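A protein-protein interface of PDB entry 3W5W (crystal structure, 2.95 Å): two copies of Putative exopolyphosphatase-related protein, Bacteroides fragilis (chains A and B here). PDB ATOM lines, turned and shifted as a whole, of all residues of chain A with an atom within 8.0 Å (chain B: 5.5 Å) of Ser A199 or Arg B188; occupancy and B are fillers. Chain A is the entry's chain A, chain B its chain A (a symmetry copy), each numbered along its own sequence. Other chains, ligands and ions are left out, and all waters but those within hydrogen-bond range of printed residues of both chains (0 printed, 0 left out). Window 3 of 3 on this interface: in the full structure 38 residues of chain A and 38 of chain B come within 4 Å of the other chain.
The backbone carbonyl oxygen of Glu A196 sits at hydrogen-bond distance from the side-chain hydroxyl of Ser A199 (2.6 Å). O of Ser B185 is in hydrogen-bond range of OH of Tyr B191, at 2.7 Å.
CB of Tyr A191 touches O of Tyr B191 (3.4 Å). Tyr B191 touches Ile A194. OD1 of Asn B186 touches CD2 of Leu A198, 3.0 Å away. Leu A198 touches Asn B187. Leu A198 touches Arg B188. Tyr B191 touches Leu A198. CB of Ser A199 touches NH1 of Arg B188, 3.1 Å away.
Printed residues of chain B within 4 Å of Ile A194: Tyr B191. Printed residues of chain B within 4 Å of Ser A195: Arg B188. Of the printed residues of chain A, Ser B185 touches Lys A204 (2.7 Å). Printed residues of chain A within 4 Å of Asn B186: Leu A198 (3.0 Å), Ile A202 (3.2 Å) and Lys A204 (3.2 Å). Arg B188 touches three residues of chain A. Printed residues of chain A within 4 Å of Tyr B191: Tyr A191, Ile A194, Leu A198 and Lys A204. The nearest printed residue of chain B that does not touch Ser A195 is Tyr B191 (4.3 Å).
The side-chain hydroxyl of Ser A195 lies within hydrogen-bond range of the guanidinium group of Arg B188 (3.1 Å). OD1 of Asn B186 lies close to O of Ile A202 (3.2 Å). The side-chain amino group (NZ) of Lys A204 is in hydrogen-bond range of the side-chain hydroxyl (OG) of Ser B185, 2.7 Å away. The side-chain amide oxygen (OD1) of Asn B186 sits at hydrogen-bond distance from the backbone NH (N) of Lys A204, 3.2 Å away. The side-chain amino group of Lys A204 lies within hydrogen-bond range of the side-chain hydroxyl of Tyr B191 (2.8 Å).
Tyr A191 touches its own counterpart, Tyr B191. 2 positions are printed for both chains.
Of the 18 printed residues of chain A, 7 touch a printed residue of chain B. Printed residues of chain A that touch a printed residue of chain B: Tyr A191, Ile A194, Ser A195, Leu A198, Ser A199, Ile A202 and Lys A204. Hydrophobic or aromatic side chains of chain A that line the printed part of chain B: Tyr A191, Ile A194 and Leu A198.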
ATOM      1  N   PHE A 159     -39.895  -2.645  17.356  1.00  0.00           N
ATOM      2  CA  PHE A 159     -38.550  -3.150  17.603  1.00  0.00           C
ATOM      3  C   PHE A 159     -37.522  -2.386  16.777  1.00  0.00           C
ATOM      4  O   PHE A 159     -36.438  -2.069  17.266  1.00  0.00           O
ATOM      5  CB  PHE A 159     -38.452  -4.638  17.275  1.00  0.00           C
ATOM      6  CG  PHE A 159     -37.050  -5.181  17.354  1.00  0.00           C
ATOM      7  CD1 PHE A 159     -36.437  -5.394  18.590  1.00  0.00           C
ATOM      8  CD2 PHE A 159     -36.325  -5.452  16.191  1.00  0.00           C
ATOM      9  CE1 PHE A 159     -35.122  -5.868  18.660  1.00  0.00           C
ATOM     10  CE2 PHE A 159     -35.014  -5.923  16.254  1.00  0.00           C
ATOM     11  CZ  PHE A 159     -34.412  -6.131  17.488  1.00  0.00           C
ATOM     12  N   ILE A 162     -36.228   1.032  18.056  1.00  0.00           N
ATOM     13  CA  ILE A 162     -35.466   1.045  19.300  1.00  0.00           C
ATOM     14  C   ILE A 162     -34.036   1.407  18.935  1.00  0.00           C
ATOM     15  O   ILE A 162     -33.354   0.640  18.247  1.00  0.00           O
ATOM     16  CB  ILE A 162     -35.491  -0.332  20.006  1.00  0.00           C
ATOM     17  CG1 ILE A 162     -36.886  -0.587  20.585  1.00  0.00           C
ATOM     18  CG2 ILE A 162     -34.419  -0.384  21.104  1.00  0.00           C
ATOM     19  CD1 ILE A 162     -37.008  -1.864  21.364  1.00  0.00           C
ATOM     20  N   SER A 163     -33.605   2.585  19.386  1.00  0.00           N
ATOM     21  CA  SER A 163     -32.266   3.103  19.121  1.00  0.00           C
ATOM     22  C   SER A 163     -31.180   2.344  19.868  1.00  0.00           C
ATOM     23  O   SER A 163     -31.471   1.474  20.687  1.00  0.00           O
ATOM     24  CB  SER A 163     -32.201   4.569  19.526  1.00  0.00           C
ATOM     25  OG  SER A 163     -32.539   4.728  20.898  1.00  0.00           O
ATOM     26  N   LYS A 164     -29.924   2.666  19.586  1.00  0.00           N
ATOM     27  CA  LYS A 164     -28.829   2.009  20.278  1.00  0.00           C
ATOM     28  C   LYS A 164     -28.812   2.541  21.703  1.00  0.00           C
ATOM     29  O   LYS A 164     -28.534   1.803  22.651  1.00  0.00           O
ATOM     30  CB  LYS A 164     -27.504   2.315  19.596  1.00  0.00           C
ATOM     31  CG  LYS A 164     -26.285   1.819  20.331  1.00  0.00           C
ATOM     32  CD  LYS A 164     -25.053   2.352  19.637  1.00  0.00           C
ATOM     33  CE  LYS A 164     -23.768   1.918  20.307  1.00  0.00           C
ATOM     34  NZ  LYS A 164     -22.623   2.029  19.354  1.00  0.00           N
ATOM     35  N   ALA A 167     -31.407   0.823  23.577  1.00  0.00           N
ATOM     36  CA  ALA A 167     -30.968  -0.550  23.807  1.00  0.00           C
ATOM     37  C   ALA A 167     -29.953  -0.611  24.938  1.00  0.00           C
ATOM     38  O   ALA A 167     -29.974  -1.534  25.743  1.00  0.00           O
ATOM     39  CB  ALA A 167     -30.364  -1.144  22.526  1.00  0.00           C
ATOM     40  N   TYR A 191     -32.070 -14.416  27.013  1.00  0.00           N
ATOM     41  CA  TYR A 191     -30.941 -14.445  26.096  1.00  0.00           C
ATOM     42  C   TYR A 191     -31.275 -14.158  24.632  1.00  0.00           C
ATOM     43  O   TYR A 191     -30.396 -13.778  23.859  1.00  0.00           O
ATOM     44  CB  TYR A 191     -30.207 -15.774  26.303  1.00  0.00           C
ATOM     45  CG  TYR A 191     -29.885 -15.903  27.772  1.00  0.00           C
ATOM     46  CD1 TYR A 191     -28.808 -15.215  28.322  1.00  0.00           C
ATOM     47  CD2 TYR A 191     -30.783 -16.519  28.649  1.00  0.00           C
ATOM     48  CE1 TYR A 191     -28.643 -15.115  29.701  1.00  0.00           C
ATOM     49  CE2 TYR A 191     -30.630 -16.426  30.034  1.00  0.00           C
ATOM     50  CZ  TYR A 191     -29.560 -15.714  30.552  1.00  0.00           C
ATOM     51  OH  TYR A 191     -29.434 -15.551  31.914  1.00  0.00           O
ATOM     52  N   PHE A 192     -32.537 -14.315  24.247  1.00  0.00           N
ATOM     53  CA  PHE A 192     -32.931 -13.997  22.880  1.00  0.00           C
ATOM     54  C   PHE A 192     -32.937 -12.475  22.808  1.00  0.00           C
ATOM     55  O   PHE A 192     -32.550 -11.878  21.793  1.00  0.00           O
ATOM     56  CB  PHE A 192     -34.333 -14.517  22.574  1.00  0.00           C
ATOM     57  CG  PHE A 192     -34.872 -14.050  21.251  1.00  0.00           C
ATOM     58  CD1 PHE A 192     -34.278 -14.456  20.062  1.00  0.00           C
ATOM     59  CD2 PHE A 192     -35.965 -13.181  21.196  1.00  0.00           C
ATOM     60  CE1 PHE A 192     -34.762 -14.005  18.833  1.00  0.00           C
ATOM     61  CE2 PHE A 192     -36.461 -12.721  19.972  1.00  0.00           C
ATOM     62  CZ  PHE A 192     -35.857 -13.137  18.790  1.00  0.00           C
ATOM     63  N   ILE A 193     -33.385 -11.860  23.905  1.00  0.00           N
ATOM     64  CA  ILE A 193     -33.453 -10.410  24.031  1.00  0.00           C
ATOM     65  C   ILE A 193     -32.044  -9.822  24.109  1.00  0.00           C
ATOM     66  O   ILE A 193     -31.772  -8.769  23.537  1.00  0.00           O
ATOM     67  CB  ILE A 193     -34.263 -10.001  25.286  1.00  0.00           C
ATOM     68  CG1 ILE A 193     -35.715 -10.428  25.116  1.00  0.00           C
ATOM     69  CG2 ILE A 193     -34.206  -8.494  25.496  1.00  0.00           C
ATOM     70  CD1 ILE A 193     -36.582 -10.036  26.273  1.00  0.00           C
ATOM     71  N   ILE A 194     -31.143 -10.494  24.816  1.00  0.00           N
ATOM     72  CA  ILE A 194     -29.779  -9.992  24.908  1.00  0.00           C
ATOM     73  C   ILE A 194     -29.204  -9.972  23.499  1.00  0.00           C
ATOM     74  O   ILE A 194     -28.590  -8.993  23.069  1.00  0.00           O
ATOM     75  CB  ILE A 194     -28.914 -10.879  25.840  1.00  0.00           C
ATOM     76  CG1 ILE A 194     -29.257 -10.564  27.304  1.00  0.00           C
ATOM     77  CG2 ILE A 194     -27.433 -10.643  25.578  1.00  0.00           C
ATOM     78  CD1 ILE A 194     -28.511 -11.394  28.322  1.00  0.00           C
ATOM     79  N   SER A 195     -29.441 -11.056  22.770  1.00  0.00           N
ATOM     80  CA  SER A 195     -28.951 -11.169  21.415  1.00  0.00           C
ATOM     81  C   SER A 195     -29.556 -10.062  20.555  1.00  0.00           C
ATOM     82  O   SER A 195     -28.872  -9.450  19.743  1.00  0.00           O
ATOM     83  CB  SER A 195     -29.301 -12.541  20.858  1.00  0.00           C
ATOM     84  OG  SER A 195     -28.477 -12.847  19.753  1.00  0.00           O
ATOM     85  N   GLU A 196     -30.837  -9.782  20.740  1.00  0.00           N
ATOM     86  CA  GLU A 196     -31.473  -8.727  19.958  1.00  0.00           C
ATOM     87  C   GLU A 196     -30.909  -7.343  20.261  1.00  0.00           C
ATOM     88  O   GLU A 196     -30.712  -6.537  19.352  1.00  0.00           O
ATOM     89  CB  GLU A 196     -32.980  -8.730  20.189  1.00  0.00           C
ATOM     90  CG  GLU A 196     -33.637  -9.966  19.633  1.00  0.00           C
ATOM     91  CD  GLU A 196     -35.026  -9.685  19.112  1.00  0.00           C
ATOM     92  OE1 GLU A 196     -35.941  -9.512  19.944  1.00  0.00           O
ATOM     93  OE2 GLU A 196     -35.196  -9.626  17.871  1.00  0.00           O
ATOM     94  N   LEU A 197     -30.649  -7.064  21.539  1.00  0.00           N
ATOM     95  CA  LEU A 197     -30.108  -5.765  21.926  1.00  0.00           C
ATOM     96  C   LEU A 197     -28.728  -5.645  21.302  1.00  0.00           C
ATOM     97  O   LEU A 197     -28.391  -4.611  20.724  1.00  0.00           O
ATOM     98  CB  LEU A 197     -30.027  -5.636  23.455  1.00  0.00           C
ATOM     99  CG  LEU A 197     -31.356  -5.748  24.221  1.00  0.00           C
ATOM    100  CD1 LEU A 197     -31.095  -5.923  25.715  1.00  0.00           C
ATOM    101  CD2 LEU A 197     -32.209  -4.521  23.957  1.00  0.00           C
ATOM    102  N   LEU A 198     -27.932  -6.707  21.395  1.00  0.00           N
ATOM    103  CA  LEU A 198     -26.595  -6.672  20.819  1.00  0.00           C
ATOM    104  C   LEU A 198     -26.635  -6.246  19.359  1.00  0.00           C
ATOM    105  O   LEU A 198     -25.713  -5.584  18.875  1.00  0.00           O
ATOM    106  CB  LEU A 198     -25.915  -8.031  20.937  1.00  0.00           C
ATOM    107  CG  LEU A 198     -25.150  -8.273  22.228  1.00  0.00           C
ATOM    108  CD1 LEU A 198     -24.416  -9.588  22.113  1.00  0.00           C
ATOM    109  CD2 LEU A 198     -24.169  -7.151  22.468  1.00  0.00           C
ATOM    110  N   SER A 199     -27.707  -6.615  18.666  1.00  0.00           N
ATOM    111  CA  SER A 199     -27.865  -6.263  17.261  1.00  0.00           C
ATOM    112  C   SER A 199     -28.274  -4.795  17.066  1.00  0.00           C
ATOM    113  O   SER A 199     -28.494  -4.369  15.932  1.00  0.00           O
ATOM    114  CB  SER A 199     -28.907  -7.158  16.602  1.00  0.00           C
ATOM    115  OG  SER A 199     -30.208  -6.637  16.813  1.00  0.00           O
ATOM    116  N   LYS A 200     -28.407  -4.036  18.157  1.00  0.00           N
ATOM    117  CA  LYS A 200     -28.740  -2.607  18.075  1.00  0.00           C
ATOM    118  C   LYS A 200     -27.424  -1.837  18.184  1.00  0.00           C
ATOM    119  O   LYS A 200     -27.391  -0.599  18.126  1.00  0.00           O
ATOM    120  CB  LYS A 200     -29.677  -2.182  19.203  1.00  0.00           C
ATOM    121  CG  LYS A 200     -31.054  -2.773  19.125  1.00  0.00           C
ATOM    122  CD  LYS A 200     -31.823  -2.178  18.000  1.00  0.00           C
ATOM    123  CE  LYS A 200     -33.187  -2.822  17.924  1.00  0.00           C
ATOM    124  NZ  LYS A 200     -34.021  -2.203  16.861  1.00  0.00           N
ATOM    125  N   GLY A 201     -26.346  -2.597  18.374  1.00  0.00           N
ATOM    126  CA  GLY A 201     -25.011  -2.029  18.443  1.00  0.00           C
ATOM    127  C   GLY A 201     -24.366  -1.802  19.790  1.00  0.00           C
ATOM    128  O   GLY A 201     -23.327  -1.156  19.858  1.00  0.00           O
ATOM    129  N   ILE A 202     -24.946  -2.325  20.860  1.00  0.00           N
ATOM    130  CA  ILE A 202     -24.358  -2.095  22.169  1.00  0.00           C
ATOM    131  C   ILE A 202     -23.168  -3.003  22.428  1.00  0.00           C
ATOM    132  O   ILE A 202     -22.976  -4.010  21.742  1.00  0.00           O
ATOM    133  CB  ILE A 202     -25.388  -2.280  23.313  1.00  0.00           C
ATOM    134  CG1 ILE A 202     -25.655  -3.756  23.570  1.00  0.00           C
ATOM    135  CG2 ILE A 202     -26.687  -1.605  22.953  1.00  0.00           C
ATOM    136  CD1 ILE A 202     -26.527  -3.991  24.773  1.00  0.00           C
ATOM    137  N   LYS A 204     -22.068  -4.981  25.409  1.00  0.00           N
ATOM    138  CA  LYS A 204     -22.427  -5.420  26.746  1.00  0.00           C
ATOM    139  C   LYS A 204     -21.237  -5.440  27.675  1.00  0.00           C
ATOM    140  O   LYS A 204     -21.350  -5.056  28.834  1.00  0.00           O
ATOM    141  CB  LYS A 204     -23.102  -6.794  26.718  1.00  0.00           C
ATOM    142  CG  LYS A 204     -22.316  -7.890  26.053  1.00  0.00           C
ATOM    143  CD  LYS A 204     -23.157  -9.161  25.988  1.00  0.00           C
ATOM    144  CE  LYS A 204     -23.428  -9.725  27.374  1.00  0.00           C
ATOM    145  NZ  LYS A 204     -22.162 -10.193  28.026  1.00  0.00           N
ATOM    146  N   SER B 185     -17.510 -11.255  25.131  1.00  0.00           N
ATOM    147  CA  SER B 185     -18.795 -11.929  25.006  1.00  0.00           C
ATOM    148  C   SER B 185     -19.813 -11.140  24.197  1.00  0.00           C
ATOM    149  O   SER B 185     -21.015 -11.421  24.249  1.00  0.00           O
ATOM    150  CB  SER B 185     -19.368 -12.192  26.398  1.00  0.00           C
ATOM    151  OG  SER B 185     -19.740 -10.973  27.014  1.00  0.00           O
ATOM    152  N   ASN B 186     -19.333 -10.164  23.437  1.00  0.00           N
ATOM    153  CA  ASN B 186     -20.214  -9.315  22.641  1.00  0.00           C
ATOM    154  C   ASN B 186     -20.858  -9.908  21.403  1.00  0.00           C
ATOM    155  O   ASN B 186     -21.624  -9.236  20.721  1.00  0.00           O
ATOM    156  CB  ASN B 186     -19.473  -8.053  22.234  1.00  0.00           C
ATOM    157  CG  ASN B 186     -20.064  -6.837  22.858  1.00  0.00           C
ATOM    158  OD1 ASN B 186     -21.255  -6.577  22.715  1.00  0.00           O
ATOM    159  ND2 ASN B 186     -19.243  -6.082  23.570  1.00  0.00           N
ATOM    160  N   ASN B 187     -20.562 -11.163  21.119  1.00  0.00           N
ATOM    161  CA  ASN B 187     -21.094 -11.824  19.946  1.00  0.00           C
ATOM    162  C   ASN B 187     -22.468 -12.464  20.201  1.00  0.00           C
ATOM    163  O   ASN B 187     -22.597 -13.343  21.044  1.00  0.00           O
ATOM    164  CB  ASN B 187     -20.053 -12.847  19.474  1.00  0.00           C
ATOM    165  CG  ASN B 187     -20.582 -13.783  18.422  1.00  0.00           C
ATOM    166  OD1 ASN B 187     -21.338 -13.379  17.525  1.00  0.00           O
ATOM    167  ND2 ASN B 187     -20.179 -15.053  18.510  1.00  0.00           N
ATOM    168  N   ARG B 188     -23.482 -12.005  19.467  1.00  0.00           N
ATOM    169  CA  ARG B 188     -24.861 -12.493  19.584  1.00  0.00           C
ATOM    170  C   ARG B 188     -25.046 -13.992  19.718  1.00  0.00           C
ATOM    171  O   ARG B 188     -25.796 -14.466  20.565  1.00  0.00           O
ATOM    172  CB  ARG B 188     -25.686 -12.094  18.364  1.00  0.00           C
ATOM    173  CG  ARG B 188     -25.747 -10.627  18.038  1.00  0.00           C
ATOM    174  CD  ARG B 188     -26.742 -10.425  16.900  1.00  0.00           C
ATOM    175  NE  ARG B 188     -27.924 -11.270  17.092  1.00  0.00           N
ATOM    176  CZ  ARG B 188     -29.091 -11.094  16.478  1.00  0.00           C
ATOM    177  NH1 ARG B 188     -29.245 -10.097  15.616  1.00  0.00           N
ATOM    178  NH2 ARG B 188     -30.109 -11.909  16.744  1.00  0.00           N
ATOM    179  N   GLU B 189     -24.388 -14.736  18.844  1.00  0.00           N
ATOM    180  CA  GLU B 189     -24.529 -16.178  18.832  1.00  0.00           C
ATOM    181  C   GLU B 189     -24.240 -16.845  20.166  1.00  0.00           C
ATOM    182  O   GLU B 189     -24.750 -17.926  20.443  1.00  0.00           O
ATOM    183  CB  GLU B 189     -23.658 -16.759  17.728  1.00  0.00           C
ATOM    184  CG  GLU B 189     -23.897 -16.084  16.392  1.00  0.00           C
ATOM    185  CD  GLU B 189     -23.320 -16.872  15.241  1.00  0.00           C
ATOM    186  OE1 GLU B 189     -23.801 -18.000  15.011  1.00  0.00           O
ATOM    187  OE2 GLU B 189     -22.384 -16.376  14.570  1.00  0.00           O
ATOM    188  N   ILE B 190     -23.426 -16.210  20.996  1.00  0.00           N
ATOM    189  CA  ILE B 190     -23.116 -16.774  22.301  1.00  0.00           C
ATOM    190  C   ILE B 190     -24.433 -16.992  23.033  1.00  0.00           C
ATOM    191  O   ILE B 190     -24.689 -18.060  23.584  1.00  0.00           O
ATOM    192  CB  ILE B 190     -22.227 -15.813  23.139  1.00  0.00           C
ATOM    193  CG1 ILE B 190     -20.763 -15.951  22.722  1.00  0.00           C
ATOM    194  CG2 ILE B 190     -22.395 -16.096  24.618  1.00  0.00           C
ATOM    195  CD1 ILE B 190     -19.838 -14.938  23.383  1.00  0.00           C
ATOM    196  N   TYR B 191     -25.282 -15.976  22.997  1.00  0.00           N
ATOM    197  CA  TYR B 191     -26.567 -16.017  23.678  1.00  0.00           C
ATOM    198  C   TYR B 191     -27.616 -16.933  23.046  1.00  0.00           C
ATOM    199  O   TYR B 191     -28.564 -17.343  23.716  1.00  0.00           O
ATOM    200  CB  TYR B 191     -27.046 -14.574  23.855  1.00  0.00           C
ATOM    201  CG  TYR B 191     -25.946 -13.800  24.539  1.00  0.00           C
ATOM    202  CD1 TYR B 191     -25.753 -13.911  25.913  1.00  0.00           C
ATOM    203  CD2 TYR B 191     -24.963 -13.144  23.792  1.00  0.00           C
ATOM    204  CE1 TYR B 191     -24.603 -13.414  26.523  1.00  0.00           C
ATOM    205  CE2 TYR B 191     -23.805 -12.643  24.391  1.00  0.00           C
ATOM    206  CZ  TYR B 191     -23.629 -12.790  25.758  1.00  0.00           C
ATOM    207  OH  TYR B 191     -22.462 -12.367  26.354  1.00  0.00           O
ATOM    208  N   PHE B 192     -27.451 -17.272  21.772  1.00  0.00           N
ATOM    209  CA  PHE B 192     -28.382 -18.192  21.133  1.00  0.00           C
ATOM    210  C   PHE B 192     -28.048 -19.565  21.703  1.00  0.00           C
ATOM    211  O   PHE B 192     -28.937 -20.389  21.957  1.00  0.00           O
ATOM    212  CB  PHE B 192     -28.183 -18.217  19.620  1.00  0.00           C
ATOM    213  CG  PHE B 192     -28.975 -19.289  18.926  1.00  0.00           C
ATOM    214  CD1 PHE B 192     -30.365 -19.244  18.911  1.00  0.00           C
ATOM    215  CD2 PHE B 192     -28.331 -20.361  18.304  1.00  0.00           C
ATOM    216  CE1 PHE B 192     -31.104 -20.249  18.288  1.00  0.00           C
ATOM    217  CE2 PHE B 192     -29.058 -21.375  17.675  1.00  0.00           C
ATOM    218  CZ  PHE B 192     -30.448 -21.317  17.667  1.00  0.00           C
